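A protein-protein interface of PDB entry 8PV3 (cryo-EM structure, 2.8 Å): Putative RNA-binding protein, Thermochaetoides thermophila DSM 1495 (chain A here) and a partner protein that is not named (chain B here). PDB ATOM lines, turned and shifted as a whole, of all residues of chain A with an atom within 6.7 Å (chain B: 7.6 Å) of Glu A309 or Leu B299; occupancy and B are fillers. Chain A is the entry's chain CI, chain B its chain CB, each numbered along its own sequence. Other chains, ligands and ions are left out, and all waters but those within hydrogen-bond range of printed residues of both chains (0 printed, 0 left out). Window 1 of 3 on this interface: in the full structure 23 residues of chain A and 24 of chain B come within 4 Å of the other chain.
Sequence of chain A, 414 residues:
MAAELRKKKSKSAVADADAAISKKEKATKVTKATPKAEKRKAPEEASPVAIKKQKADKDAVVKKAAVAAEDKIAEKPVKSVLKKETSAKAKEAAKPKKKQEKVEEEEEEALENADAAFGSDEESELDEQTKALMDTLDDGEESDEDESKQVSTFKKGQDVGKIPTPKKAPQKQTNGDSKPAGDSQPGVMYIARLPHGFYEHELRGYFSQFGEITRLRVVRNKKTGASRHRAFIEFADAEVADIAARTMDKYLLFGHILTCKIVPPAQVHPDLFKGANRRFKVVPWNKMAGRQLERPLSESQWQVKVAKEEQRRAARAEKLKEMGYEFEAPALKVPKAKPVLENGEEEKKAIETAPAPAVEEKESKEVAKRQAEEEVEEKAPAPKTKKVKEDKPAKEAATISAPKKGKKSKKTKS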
ATOM      1  N   TRP A 302     -32.411   1.442   2.699  1.00  0.00           N
ATOM      2  CA  TRP A 302     -31.009   1.026   2.798  1.00  0.00           C
ATOM      3  C   TRP A 302     -30.506   0.386   1.494  1.00  0.00           C
ATOM      4  O   TRP A 302     -29.398   0.706   1.034  1.00  0.00           O
ATOM      5  CB  TRP A 302     -30.813   0.113   4.009  1.00  0.00           C
ATOM      6  CG  TRP A 302     -30.738   0.879   5.310  1.00  0.00           C
ATOM      7  CD1 TRP A 302     -31.628   1.809   5.765  1.00  0.00           C
ATOM      8  CD2 TRP A 302     -29.765   0.723   6.351  1.00  0.00           C
ATOM      9  NE1 TRP A 302     -31.252   2.268   7.001  1.00  0.00           N
ATOM     10  CE2 TRP A 302     -30.113   1.616   7.385  1.00  0.00           C
ATOM     11  CE3 TRP A 302     -28.625  -0.070   6.501  1.00  0.00           C
ATOM     12  CZ2 TRP A 302     -29.364   1.736   8.552  1.00  0.00           C
ATOM     13  CZ3 TRP A 302     -27.882   0.052   7.663  1.00  0.00           C
ATOM     14  CH2 TRP A 302     -28.256   0.947   8.673  1.00  0.00           C
ATOM     15  N   VAL A 304     -31.854   1.131  -1.340  1.00  0.00           N
ATOM     16  CA  VAL A 304     -31.891   2.288  -2.242  1.00  0.00           C
ATOM     17  C   VAL A 304     -30.607   3.109  -2.122  1.00  0.00           C
ATOM     18  O   VAL A 304     -30.004   3.503  -3.131  1.00  0.00           O
ATOM     19  CB  VAL A 304     -33.138   3.152  -1.978  1.00  0.00           C
ATOM     20  CG1 VAL A 304     -33.107   4.404  -2.837  1.00  0.00           C
ATOM     21  CG2 VAL A 304     -34.396   2.366  -2.290  1.00  0.00           C
ATOM     22  N   LYS A 305     -30.147   3.347  -0.890  1.00  0.00           N
ATOM     23  CA  LYS A 305     -28.976   4.197  -0.710  1.00  0.00           C
ATOM     24  C   LYS A 305     -27.696   3.482  -1.130  1.00  0.00           C
ATOM     25  O   LYS A 305     -26.808   4.107  -1.725  1.00  0.00           O
ATOM     26  CB  LYS A 305     -28.888   4.715   0.733  1.00  0.00           C
ATOM     27  CG  LYS A 305     -28.602   3.694   1.818  1.00  0.00           C
ATOM     28  CD  LYS A 305     -28.563   4.345   3.192  1.00  0.00           C
ATOM     29  CE  LYS A 305     -28.319   3.317   4.285  1.00  0.00           C
ATOM     30  NZ  LYS A 305     -26.962   2.717   4.193  1.00  0.00           N
ATOM     31  N   VAL A 306     -27.592   2.167  -0.888  1.00  0.00           N
ATOM     32  CA  VAL A 306     -26.390   1.467  -1.347  1.00  0.00           C
ATOM     33  C   VAL A 306     -26.401   1.347  -2.870  1.00  0.00           C
ATOM     34  O   VAL A 306     -25.347   1.376  -3.517  1.00  0.00           O
ATOM     35  CB  VAL A 306     -26.227   0.095  -0.658  1.00  0.00           C
ATOM     36  CG1 VAL A 306     -26.080   0.254   0.851  1.00  0.00           C
ATOM     37  CG2 VAL A 306     -27.321  -0.881  -1.022  1.00  0.00           C
ATOM     38  N   ALA A 307     -27.593   1.274  -3.474  1.00  0.00           N
ATOM     39  CA  ALA A 307     -27.684   1.235  -4.929  1.00  0.00           C
ATOM     40  C   ALA A 307     -27.242   2.557  -5.545  1.00  0.00           C
ATOM     41  O   ALA A 307     -26.425   2.575  -6.476  1.00  0.00           O
ATOM     42  CB  ALA A 307     -29.112   0.891  -5.354  1.00  0.00           C
ATOM     43  N   LYS A 308     -27.763   3.675  -5.028  1.00  0.00           N
ATOM     44  CA  LYS A 308     -27.381   4.975  -5.573  1.00  0.00           C
ATOM     45  C   LYS A 308     -25.907   5.261  -5.308  1.00  0.00           C
ATOM     46  O   LYS A 308     -25.235   5.911  -6.118  1.00  0.00           O
ATOM     47  CB  LYS A 308     -28.306   6.078  -5.037  1.00  0.00           C
ATOM     48  CG  LYS A 308     -28.289   6.368  -3.539  1.00  0.00           C
ATOM     49  CD  LYS A 308     -27.283   7.431  -3.112  1.00  0.00           C
ATOM     50  CE  LYS A 308     -27.419   7.727  -1.626  1.00  0.00           C
ATOM     51  NZ  LYS A 308     -26.442   8.744  -1.162  1.00  0.00           N
ATOM     52  N   GLU A 309     -25.366   4.713  -4.212  1.00  0.00           N
ATOM     53  CA  GLU A 309     -23.919   4.722  -4.027  1.00  0.00           C
ATOM     54  C   GLU A 309     -23.216   3.909  -5.109  1.00  0.00           C
ATOM     55  O   GLU A 309     -22.115   4.267  -5.541  1.00  0.00           O
ATOM     56  CB  GLU A 309     -23.549   4.183  -2.646  1.00  0.00           C
ATOM     57  CG  GLU A 309     -22.079   4.389  -2.299  1.00  0.00           C
ATOM     58  CD  GLU A 309     -21.779   4.188  -0.831  1.00  0.00           C
ATOM     59  OE1 GLU A 309     -21.115   3.186  -0.495  1.00  0.00           O
ATOM     60  OE2 GLU A 309     -22.201   5.031  -0.016  1.00  0.00           O
ATOM     61  N   GLU A 310     -23.830   2.803  -5.549  1.00  0.00           N
ATOM     62  CA  GLU A 310     -23.211   1.991  -6.595  1.00  0.00           C
ATOM     63  C   GLU A 310     -23.088   2.760  -7.909  1.00  0.00           C
ATOM     64  O   GLU A 310     -22.010   2.766  -8.519  1.00  0.00           O
ATOM     65  CB  GLU A 310     -23.980   0.684  -6.805  1.00  0.00           C
ATOM     66  CG  GLU A 310     -23.684  -0.398  -5.778  1.00  0.00           C
ATOM     67  CD  GLU A 310     -22.261  -0.910  -5.863  1.00  0.00           C
ATOM     68  OE1 GLU A 310     -21.720  -0.976  -6.987  1.00  0.00           O
ATOM     69  OE2 GLU A 310     -21.684  -1.243  -4.807  1.00  0.00           O
ATOM     70  N   GLN A 311     -24.155   3.441  -8.362  1.00  0.00           N
ATOM     71  CA  GLN A 311     -23.939   4.181  -9.616  1.00  0.00           C
ATOM     72  C   GLN A 311     -23.151   5.470  -9.384  1.00  0.00           C
ATOM     73  O   GLN A 311     -22.534   5.983 -10.322  1.00  0.00           O
ATOM     74  CB  GLN A 311     -25.184   4.526 -10.463  1.00  0.00           C
ATOM     75  CG  GLN A 311     -26.210   5.557  -9.997  1.00  0.00           C
ATOM     76  CD  GLN A 311     -27.275   4.996  -9.123  1.00  0.00           C
ATOM     77  OE1 GLN A 311     -27.140   3.911  -8.609  1.00  0.00           O
ATOM     78  NE2 GLN A 311     -28.358   5.743  -8.949  1.00  0.00           N
ATOM     79  N   ARG A 312     -23.126   6.001  -8.153  1.00  0.00           N
ATOM     80  CA  ARG A 312     -22.228   7.125  -7.886  1.00  0.00           C
ATOM     81  C   ARG A 312     -20.768   6.707  -8.035  1.00  0.00           C
ATOM     82  O   ARG A 312     -19.976   7.401  -8.690  1.00  0.00           O
ATOM     83  CB  ARG A 312     -22.475   7.705  -6.491  1.00  0.00           C
ATOM     84  CG  ARG A 312     -21.289   8.517  -5.963  1.00  0.00           C
ATOM     85  CD  ARG A 312     -21.694   9.613  -4.993  1.00  0.00           C
ATOM     86  NE  ARG A 312     -22.433   9.113  -3.842  1.00  0.00           N
ATOM     87  CZ  ARG A 312     -22.920   9.884  -2.880  1.00  0.00           C
ATOM     88  NH1 ARG A 312     -22.802  11.202  -2.925  1.00  0.00           N
ATOM     89  NH2 ARG A 312     -23.542   9.321  -1.849  1.00  0.00           N
ATOM     90  N   ARG A 313     -20.405   5.556  -7.464  1.00  0.00           N
ATOM     91  CA  ARG A 313     -19.043   5.050  -7.595  1.00  0.00           C
ATOM     92  C   ARG A 313     -18.737   4.668  -9.036  1.00  0.00           C
ATOM     93  O   ARG A 313     -17.612   4.863  -9.509  1.00  0.00           O
ATOM     94  CB  ARG A 313     -18.830   3.845  -6.681  1.00  0.00           C
ATOM     95  CG  ARG A 313     -18.853   4.157  -5.202  1.00  0.00           C
ATOM     96  CD  ARG A 313     -18.580   2.905  -4.391  1.00  0.00           C
ATOM     97  NE  ARG A 313     -18.535   3.184  -2.961  1.00  0.00           N
ATOM     98  CZ  ARG A 313     -18.205   2.295  -2.033  1.00  0.00           C
ATOM     99  NH1 ARG A 313     -17.792   1.080  -2.355  1.00  0.00           N
ATOM    100  NH2 ARG A 313     -18.276   2.641  -0.752  1.00  0.00           N
ATOM    101  N   ALA A 314     -19.729   4.128  -9.751  1.00  0.00           N
ATOM    102  CA  ALA A 314     -19.539   3.812 -11.163  1.00  0.00           C
ATOM    103  C   ALA A 314     -19.279   5.069 -11.985  1.00  0.00           C
ATOM    104  O   ALA A 314     -18.363   5.098 -12.817  1.00  0.00           O
ATOM    105  CB  ALA A 314     -20.759   3.064 -11.698  1.00  0.00           C
ATOM    106  N   ARG A 316     -18.134   7.951 -10.928  1.00  0.00           N
ATOM    107  CA  ARG A 316     -16.789   8.391 -10.584  1.00  0.00           C
ATOM    108  C   ARG A 316     -15.737   7.512 -11.249  1.00  0.00           C
ATOM    109  O   ARG A 316     -14.632   7.973 -11.542  1.00  0.00           O
ATOM    110  CB  ARG A 316     -16.613   8.412  -9.064  1.00  0.00           C
ATOM    111  CG  ARG A 316     -17.365   9.551  -8.394  1.00  0.00           C
ATOM    112  CD  ARG A 316     -17.087   9.637  -6.902  1.00  0.00           C
ATOM    113  NE  ARG A 316     -17.665   8.528  -6.153  1.00  0.00           N
ATOM    114  CZ  ARG A 316     -17.536   8.365  -4.843  1.00  0.00           C
ATOM    115  NH1 ARG A 316     -16.857   9.227  -4.105  1.00  0.00           N
ATOM    116  NH2 ARG A 316     -18.103   7.314  -4.260  1.00  0.00           N
ATOM    117  N   LEU A 332     -20.867  -3.232  -2.050  1.00  0.00           N
ATOM    118  CA  LEU A 332     -21.631  -3.033  -0.824  1.00  0.00           C
ATOM    119  C   LEU A 332     -22.466  -4.271  -0.538  1.00  0.00           C
ATOM    120  O   LEU A 332     -23.284  -4.677  -1.367  1.00  0.00           O
ATOM    121  CB  LEU A 332     -22.543  -1.807  -0.947  1.00  0.00           C
ATOM    122  CG  LEU A 332     -22.037  -0.374  -0.695  1.00  0.00           C
ATOM    123  CD1 LEU A 332     -21.554  -0.197   0.745  1.00  0.00           C
ATOM    124  CD2 LEU A 332     -20.967   0.051  -1.681  1.00  0.00           C
ATOM    125  N   THR B  68     -17.193  11.140   6.605  1.00  0.00           N
ATOM    126  CA  THR B  68     -17.699  10.310   7.685  1.00  0.00           C
ATOM    127  C   THR B  68     -19.195  10.085   7.508  1.00  0.00           C
ATOM    128  O   THR B  68     -19.829  10.624   6.597  1.00  0.00           O
ATOM    129  CB  THR B  68     -17.413  10.948   9.050  1.00  0.00           C
ATOM    130  OG1 THR B  68     -17.697  12.351   8.994  1.00  0.00           O
ATOM    131  CG2 THR B  68     -15.956  10.745   9.433  1.00  0.00           C
ATOM    132  N   LYS B  69     -19.754   9.265   8.397  1.00  0.00           N
ATOM    133  CA  LYS B  69     -21.177   8.958   8.350  1.00  0.00           C
ATOM    134  C   LYS B  69     -22.019   9.962   9.121  1.00  0.00           C
ATOM    135  O   LYS B  69     -23.171  10.204   8.744  1.00  0.00           O
ATOM    136  CB  LYS B  69     -21.418   7.551   8.892  1.00  0.00           C
ATOM    137  CG  LYS B  69     -20.680   6.479   8.118  1.00  0.00           C
ATOM    138  CD  LYS B  69     -20.639   5.168   8.871  1.00  0.00           C
ATOM    139  CE  LYS B  69     -19.902   4.121   8.063  1.00  0.00           C
ATOM    140  NZ  LYS B  69     -19.817   2.816   8.774  1.00  0.00           N
ATOM    141  N   LYS B  70     -21.478  10.548  10.186  1.00  0.00           N
ATOM    142  CA  LYS B  70     -22.160  11.584  10.943  1.00  0.00           C
ATOM    143  C   LYS B  70     -21.255  12.802  11.051  1.00  0.00           C
ATOM    144  O   LYS B  70     -20.144  12.822  10.515  1.00  0.00           O
ATOM    145  CB  LYS B  70     -22.561  11.096  12.343  1.00  0.00           C
ATOM    146  CG  LYS B  70     -21.398  10.927  13.307  1.00  0.00           C
ATOM    147  CD  LYS B  70     -21.892  10.637  14.712  1.00  0.00           C
ATOM    148  CE  LYS B  70     -20.751  10.610  15.708  1.00  0.00           C
ATOM    149  NZ  LYS B  70     -21.244  10.398  17.098  1.00  0.00           N
ATOM    150  N   GLN B 276     -15.369   2.735  12.185  1.00  0.00           N
ATOM    151  CA  GLN B 276     -16.718   2.466  11.690  1.00  0.00           C
ATOM    152  C   GLN B 276     -17.540   3.747  11.575  1.00  0.00           C
ATOM    153  O   GLN B 276     -18.672   3.730  11.083  1.00  0.00           O
ATOM    154  CB  GLN B 276     -17.433   1.419  12.555  1.00  0.00           C
ATOM    155  CG  GLN B 276     -17.824   1.838  13.958  1.00  0.00           C
ATOM    156  CD  GLN B 276     -16.701   1.664  14.958  1.00  0.00           C
ATOM    157  OE1 GLN B 276     -15.536   1.517  14.589  1.00  0.00           O
ATOM    158  NE2 GLN B 276     -17.048   1.689  16.239  1.00  0.00           N
ATOM    159  N   ASN B 277     -16.991   4.868  12.049  1.00  0.00           N
ATOM    160  CA  ASN B 277     -17.530   6.172  11.678  1.00  0.00           C
ATOM    161  C   ASN B 277     -17.005   6.593  10.306  1.00  0.00           C
ATOM    162  O   ASN B 277     -17.717   7.242   9.531  1.00  0.00           O
ATOM    163  CB  ASN B 277     -17.156   7.199  12.753  1.00  0.00           C
ATOM    164  CG  ASN B 277     -17.839   8.556  12.570  1.00  0.00           C
ATOM    165  OD1 ASN B 277     -18.626   8.771  11.650  1.00  0.00           O
ATOM    166  ND2 ASN B 277     -17.525   9.483  13.466  1.00  0.00           N
ATOM    167  N   VAL B 278     -15.775   6.192   9.977  1.00  0.00           N
ATOM    168  CA  VAL B 278     -15.080   6.622   8.767  1.00  0.00           C
ATOM    169  C   VAL B 278     -15.744   6.052   7.520  1.00  0.00           C
ATOM    170  O   VAL B 278     -15.962   4.839   7.416  1.00  0.00           O
ATOM    171  CB  VAL B 278     -13.595   6.217   8.822  1.00  0.00           C
ATOM    172  CG1 VAL B 278     -12.919   6.472   7.491  1.00  0.00           C
ATOM    173  CG2 VAL B 278     -12.885   6.963   9.937  1.00  0.00           C
ATOM    174  N   ARG B 279     -16.065   6.926   6.562  1.00  0.00           N
ATOM    175  CA  ARG B 279     -16.689   6.471   5.324  1.00  0.00           C
ATOM    176  C   ARG B 279     -15.689   6.426   4.173  1.00  0.00           C
ATOM    177  O   ARG B 279     -15.478   5.368   3.571  1.00  0.00           O
ATOM    178  CB  ARG B 279     -17.873   7.373   4.978  1.00  0.00           C
ATOM    179  CG  ARG B 279     -18.754   6.887   3.842  1.00  0.00           C
ATOM    180  CD  ARG B 279     -19.829   7.920   3.552  1.00  0.00           C
ATOM    181  NE  ARG B 279     -20.817   7.469   2.580  1.00  0.00           N
ATOM    182  CZ  ARG B 279     -20.681   7.586   1.266  1.00  0.00           C
ATOM    183  NH1 ARG B 279     -19.572   8.063   0.727  1.00  0.00           N
ATOM    184  NH2 ARG B 279     -21.683   7.218   0.475  1.00  0.00           N
ATOM    185  N   ASN B 280     -15.065   7.559   3.843  1.00  0.00           N
ATOM    186  CA  ASN B 280     -14.245   7.637   2.639  1.00  0.00           C
ATOM    187  C   ASN B 280     -13.019   8.511   2.877  1.00  0.00           C
ATOM    188  O   ASN B 280     -13.023   9.414   3.719  1.00  0.00           O
ATOM    189  CB  ASN B 280     -15.042   8.191   1.451  1.00  0.00           C
ATOM    190  CG  ASN B 280     -16.163   7.271   1.006  1.00  0.00           C
ATOM    191  OD1 ASN B 280     -17.228   7.731   0.593  1.00  0.00           O
ATOM    192  ND2 ASN B 280     -15.925   5.969   1.072  1.00  0.00           N
ATOM    193  N   GLN B 295     -12.607   3.279   0.402  1.00  0.00           N
ATOM    194  CA  GLN B 295     -14.036   3.165   0.658  1.00  0.00           C
ATOM    195  C   GLN B 295     -14.272   2.119   1.733  1.00  0.00           C
ATOM    196  O   GLN B 295     -13.428   1.259   1.995  1.00  0.00           O
ATOM    197  CB  GLN B 295     -14.849   2.791  -0.589  1.00  0.00           C
ATOM    198  CG  GLN B 295     -15.212   3.935  -1.512  1.00  0.00           C
ATOM    199  CD  GLN B 295     -14.119   4.342  -2.456  1.00  0.00           C
ATOM    200  OE1 GLN B 295     -13.135   3.630  -2.645  1.00  0.00           O
ATOM    201  NE2 GLN B 295     -14.315   5.480  -3.100  1.00  0.00           N
ATOM    202  N   THR B 296     -15.442   2.203   2.350  1.00  0.00           N
ATOM    203  CA  THR B 296     -15.880   1.264   3.364  1.00  0.00           C
ATOM    204  C   THR B 296     -16.882   0.281   2.763  1.00  0.00           C
ATOM    205  O   THR B 296     -17.383   0.467   1.647  1.00  0.00           O
ATOM    206  CB  THR B 296     -16.477   2.018   4.554  1.00  0.00           C
ATOM    207  OG1 THR B 296     -16.792   1.093   5.601  1.00  0.00           O
ATOM    208  CG2 THR B 296     -17.735   2.757   4.132  1.00  0.00           C
ATOM    209  N   ASP B 297     -17.181  -0.764   3.513  1.00  0.00           N
ATOM    210  CA  ASP B 297     -18.167  -1.763   3.120  1.00  0.00           C
ATOM    211  C   ASP B 297     -19.479  -1.607   3.875  1.00  0.00           C
ATOM    212  O   ASP B 297     -20.536  -1.940   3.337  1.00  0.00           O
ATOM    213  CB  ASP B 297     -17.600  -3.178   3.329  1.00  0.00           C
ATOM    214  CG  ASP B 297     -18.611  -4.266   3.016  1.00  0.00           C
ATOM    215  OD1 ASP B 297     -19.134  -4.289   1.880  1.00  0.00           O
ATOM    216  OD2 ASP B 297     -18.897  -5.085   3.913  1.00  0.00           O
ATOM    217  N   GLU B 298     -19.437  -1.107   5.105  1.00  0.00           N
ATOM    218  CA  GLU B 298     -20.649  -0.811   5.858  1.00  0.00           C
ATOM    219  C   GLU B 298     -20.842   0.700   5.916  1.00  0.00           C
ATOM    220  O   GLU B 298     -19.906   1.432   6.252  1.00  0.00           O
ATOM    221  CB  GLU B 298     -20.553  -1.398   7.263  1.00  0.00           C
ATOM    222  CG  GLU B 298     -20.209  -2.880   7.300  1.00  0.00           C
ATOM    223  CD  GLU B 298     -20.127  -3.424   8.713  1.00  0.00           C
ATOM    224  OE1 GLU B 298     -20.258  -2.629   9.669  1.00  0.00           O
ATOM    225  OE2 GLU B 298     -19.957  -4.652   8.869  1.00  0.00           O
ATOM    226  N   LEU B 299     -22.045   1.168   5.590  1.00  0.00           N
ATOM    227  CA  LEU B 299     -22.356   2.592   5.573  1.00  0.00           C
ATOM    228  C   LEU B 299     -23.052   3.055   6.839  1.00  0.00           C
ATOM    229  O   LEU B 299     -23.600   4.161   6.868  1.00  0.00           O
ATOM    230  CB  LEU B 299     -23.220   2.931   4.362  1.00  0.00           C
ATOM    231  CG  LEU B 299     -22.615   2.568   3.015  1.00  0.00           C
ATOM    232  CD1 LEU B 299     -23.636   2.792   1.917  1.00  0.00           C
ATOM    233  CD2 LEU B 299     -21.364   3.394   2.783  1.00  0.00           C
ATOM    234  N   TRP B 300     -23.045   2.237   7.881  1.00  0.00           N
ATOM    235  CA  TRP B 300     -23.727   2.543   9.125  1.00  0.00           C
ATOM    236  C   TRP B 300     -22.732   2.559  10.278  1.00  0.00           C
ATOM    237  O   TRP B 300     -21.755   1.805  10.279  1.00  0.00           O
ATOM    238  CB  TRP B 300     -24.832   1.520   9.395  1.00  0.00           C
ATOM    239  CG  TRP B 300     -24.400   0.074   9.255  1.00  0.00           C
ATOM    240  CD1 TRP B 300     -23.979  -0.737  10.255  1.00  0.00           C
ATOM    241  CD2 TRP B 300     -24.348  -0.715   8.057  1.00  0.00           C
ATOM    242  NE1 TRP B 300     -23.674  -1.985   9.772  1.00  0.00           N
ATOM    243  CE2 TRP B 300     -23.891  -1.994   8.419  1.00  0.00           C
ATOM    244  CE3 TRP B 300     -24.643  -0.465   6.714  1.00  0.00           C
ATOM    245  CZ2 TRP B 300     -23.730  -3.021   7.489  1.00  0.00           C
ATOM    246  CZ3 TRP B 300     -24.481  -1.483   5.792  1.00  0.00           C
ATOM    247  CH2 TRP B 300     -24.023  -2.752   6.188  1.00  0.00           C
ATOM    248  N   LEU B 301     -22.982   3.437  11.257  1.00  0.00           N
ATOM    249  CA  LEU B 301     -22.116   3.507  12.433  1.00  0.00           C
ATOM    250  C   LEU B 301     -22.183   2.221  13.244  1.00  0.00           C
ATOM    251  O   LEU B 301     -21.154   1.706  13.697  1.00  0.00           O
ATOM    252  CB  LEU B 301     -22.500   4.705  13.303  1.00  0.00           C
ATOM    253  CG  LEU B 301     -21.658   4.979  14.552  1.00  0.00           C
ATOM    254  CD1 LEU B 301     -20.223   5.294  14.160  1.00  0.00           C
ATOM    255  CD2 LEU B 301     -22.272   6.114  15.368  1.00  0.00           C
ATOM    256  N   ASP B 302     -23.383   1.676  13.420  1.00  0.00           N
ATOM    257  CA  ASP B 302     -23.565   0.455  14.190  1.00  0.00           C
ATOM    258  C   ASP B 302     -24.816  -0.248  13.681  1.00  0.00           C
ATOM    259  O   ASP B 302     -25.549   0.276  12.839  1.00  0.00           O
ATOM    260  CB  ASP B 302     -23.656   0.756  15.690  1.00  0.00           C
ATOM    261  CG  ASP B 302     -24.761   1.738  16.029  1.00  0.00           C
ATOM    262  OD1 ASP B 302     -25.213   2.490  15.136  1.00  0.00           O
ATOM    263  OD2 ASP B 302     -25.176   1.751  17.206  1.00  0.00           O
ATOM    264  N   LYS B 305     -28.784   1.085  13.844  1.00  0.00           N
ATOM    265  CA  LYS B 305     -29.456   1.861  12.807  1.00  0.00           C
ATOM    266  C   LYS B 305     -30.313   0.971  11.915  1.00  0.00           C
ATOM    267  O   LYS B 305     -31.240   1.452  11.252  1.00  0.00           O
ATOM    268  CB  LYS B 305     -28.426   2.624  11.971  1.00  0.00           C
ATOM    269  CG  LYS B 305     -27.544   3.641  12.721  1.00  0.00           C
ATOM    270  CD  LYS B 305     -28.272   4.921  13.166  1.00  0.00           C
ATOM    271  CE  LYS B 305     -28.774   4.874  14.610  1.00  0.00           C
ATOM    272  NZ  LYS B 305     -29.370   6.170  15.035  1.00  0.00           N
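The guanidinium group (NE) of Arg B279 is in salt-bridge range of the side-chain carboxylate (OE2) of Glu A309 (3.8 Å). The backbone carbonyl oxygen (O) of Thr B296 sits at hydrogen-bond distance from the guanidinium group (NH2) of Arg A313 (3.4 Å).
NZ of Lys B69 is in hydrogen-bond range of O of Trp B300. The backbone carbonyl oxygen (O) of Arg B279 sits at hydrogen-bond distance from the backbone NH (N) of Thr B296 (3.4 Å). O of Glu B298 sits at hydrogen-bond distance from OG1 of Thr B296 (3.2 Å). The indole nitrogen (NE1) of Trp B300 sits at hydrogen-bond distance from the side-chain carboxylate (OE1) of Glu B298, at 3.5 Å. The side-chain carboxylate (OE1) of Glu A309 is in salt-bridge range of the guanidinium group (NH2) of Arg A313, 2.9 Å away. OE2 of Glu A310 lies close to N of Leu A332 (3.5 Å).
Trp A302 touches Trp B300. Lys B305 touches Trp A302. Lys A305 touches Leu B299 (NZ to CB, 3.8 Å). Val A306 touches Leu B299 (CG1 to CD1, 3.7 Å). OE2 of Glu A309 touches CD1 of Leu B299, 3.3 Å away. Arg A312 touches Arg B279 (NH2 to NH2, 3.6 Å). Arg A313 touches Gln B295. Leu A332 touches Asp B297. CD1 of Leu A332 touches CG of Leu B299 (3.7 Å).
Glu A309 touches just these residues of chain B: Arg B279 (2.3 Å) and Leu B299 (3.3 Å). Leu B299 touches just these residues of chain A: Lys A305 (3.8 Å), Val A306 (3.7 Å), Glu A309 (3.3 Å) and Leu A332 (3.7 Å). Printed residues of chain A within 4 Å of Gln B295: Arg A313. Printed residues of chain B within 4 Å of Lys A305: Leu B299. Of the printed residues of chain B, Arg A313 touches Gln B295 (3.4 Å) and Thr B296 (3.4 Å). The nearest residue of chain B that does not touch Glu A309 is Thr B296 (5.1 Å). The nearest printed residue of chain A that does not touch Lys B305 is Lys A305 (7.7 Å).
Of the 14 printed residues of chain A, 7 touch a printed residue of chain B. Hydrophobic or aromatic side chains of chain A within 4 Å of the printed part of chain B: Trp A302, Val A306 and Leu A332. Hydrophobic or aromatic side chains of chain B that line the printed part of chain A: Leu B299 and Trp B300. Among the printed residues, 11 pairs touch across the chains.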
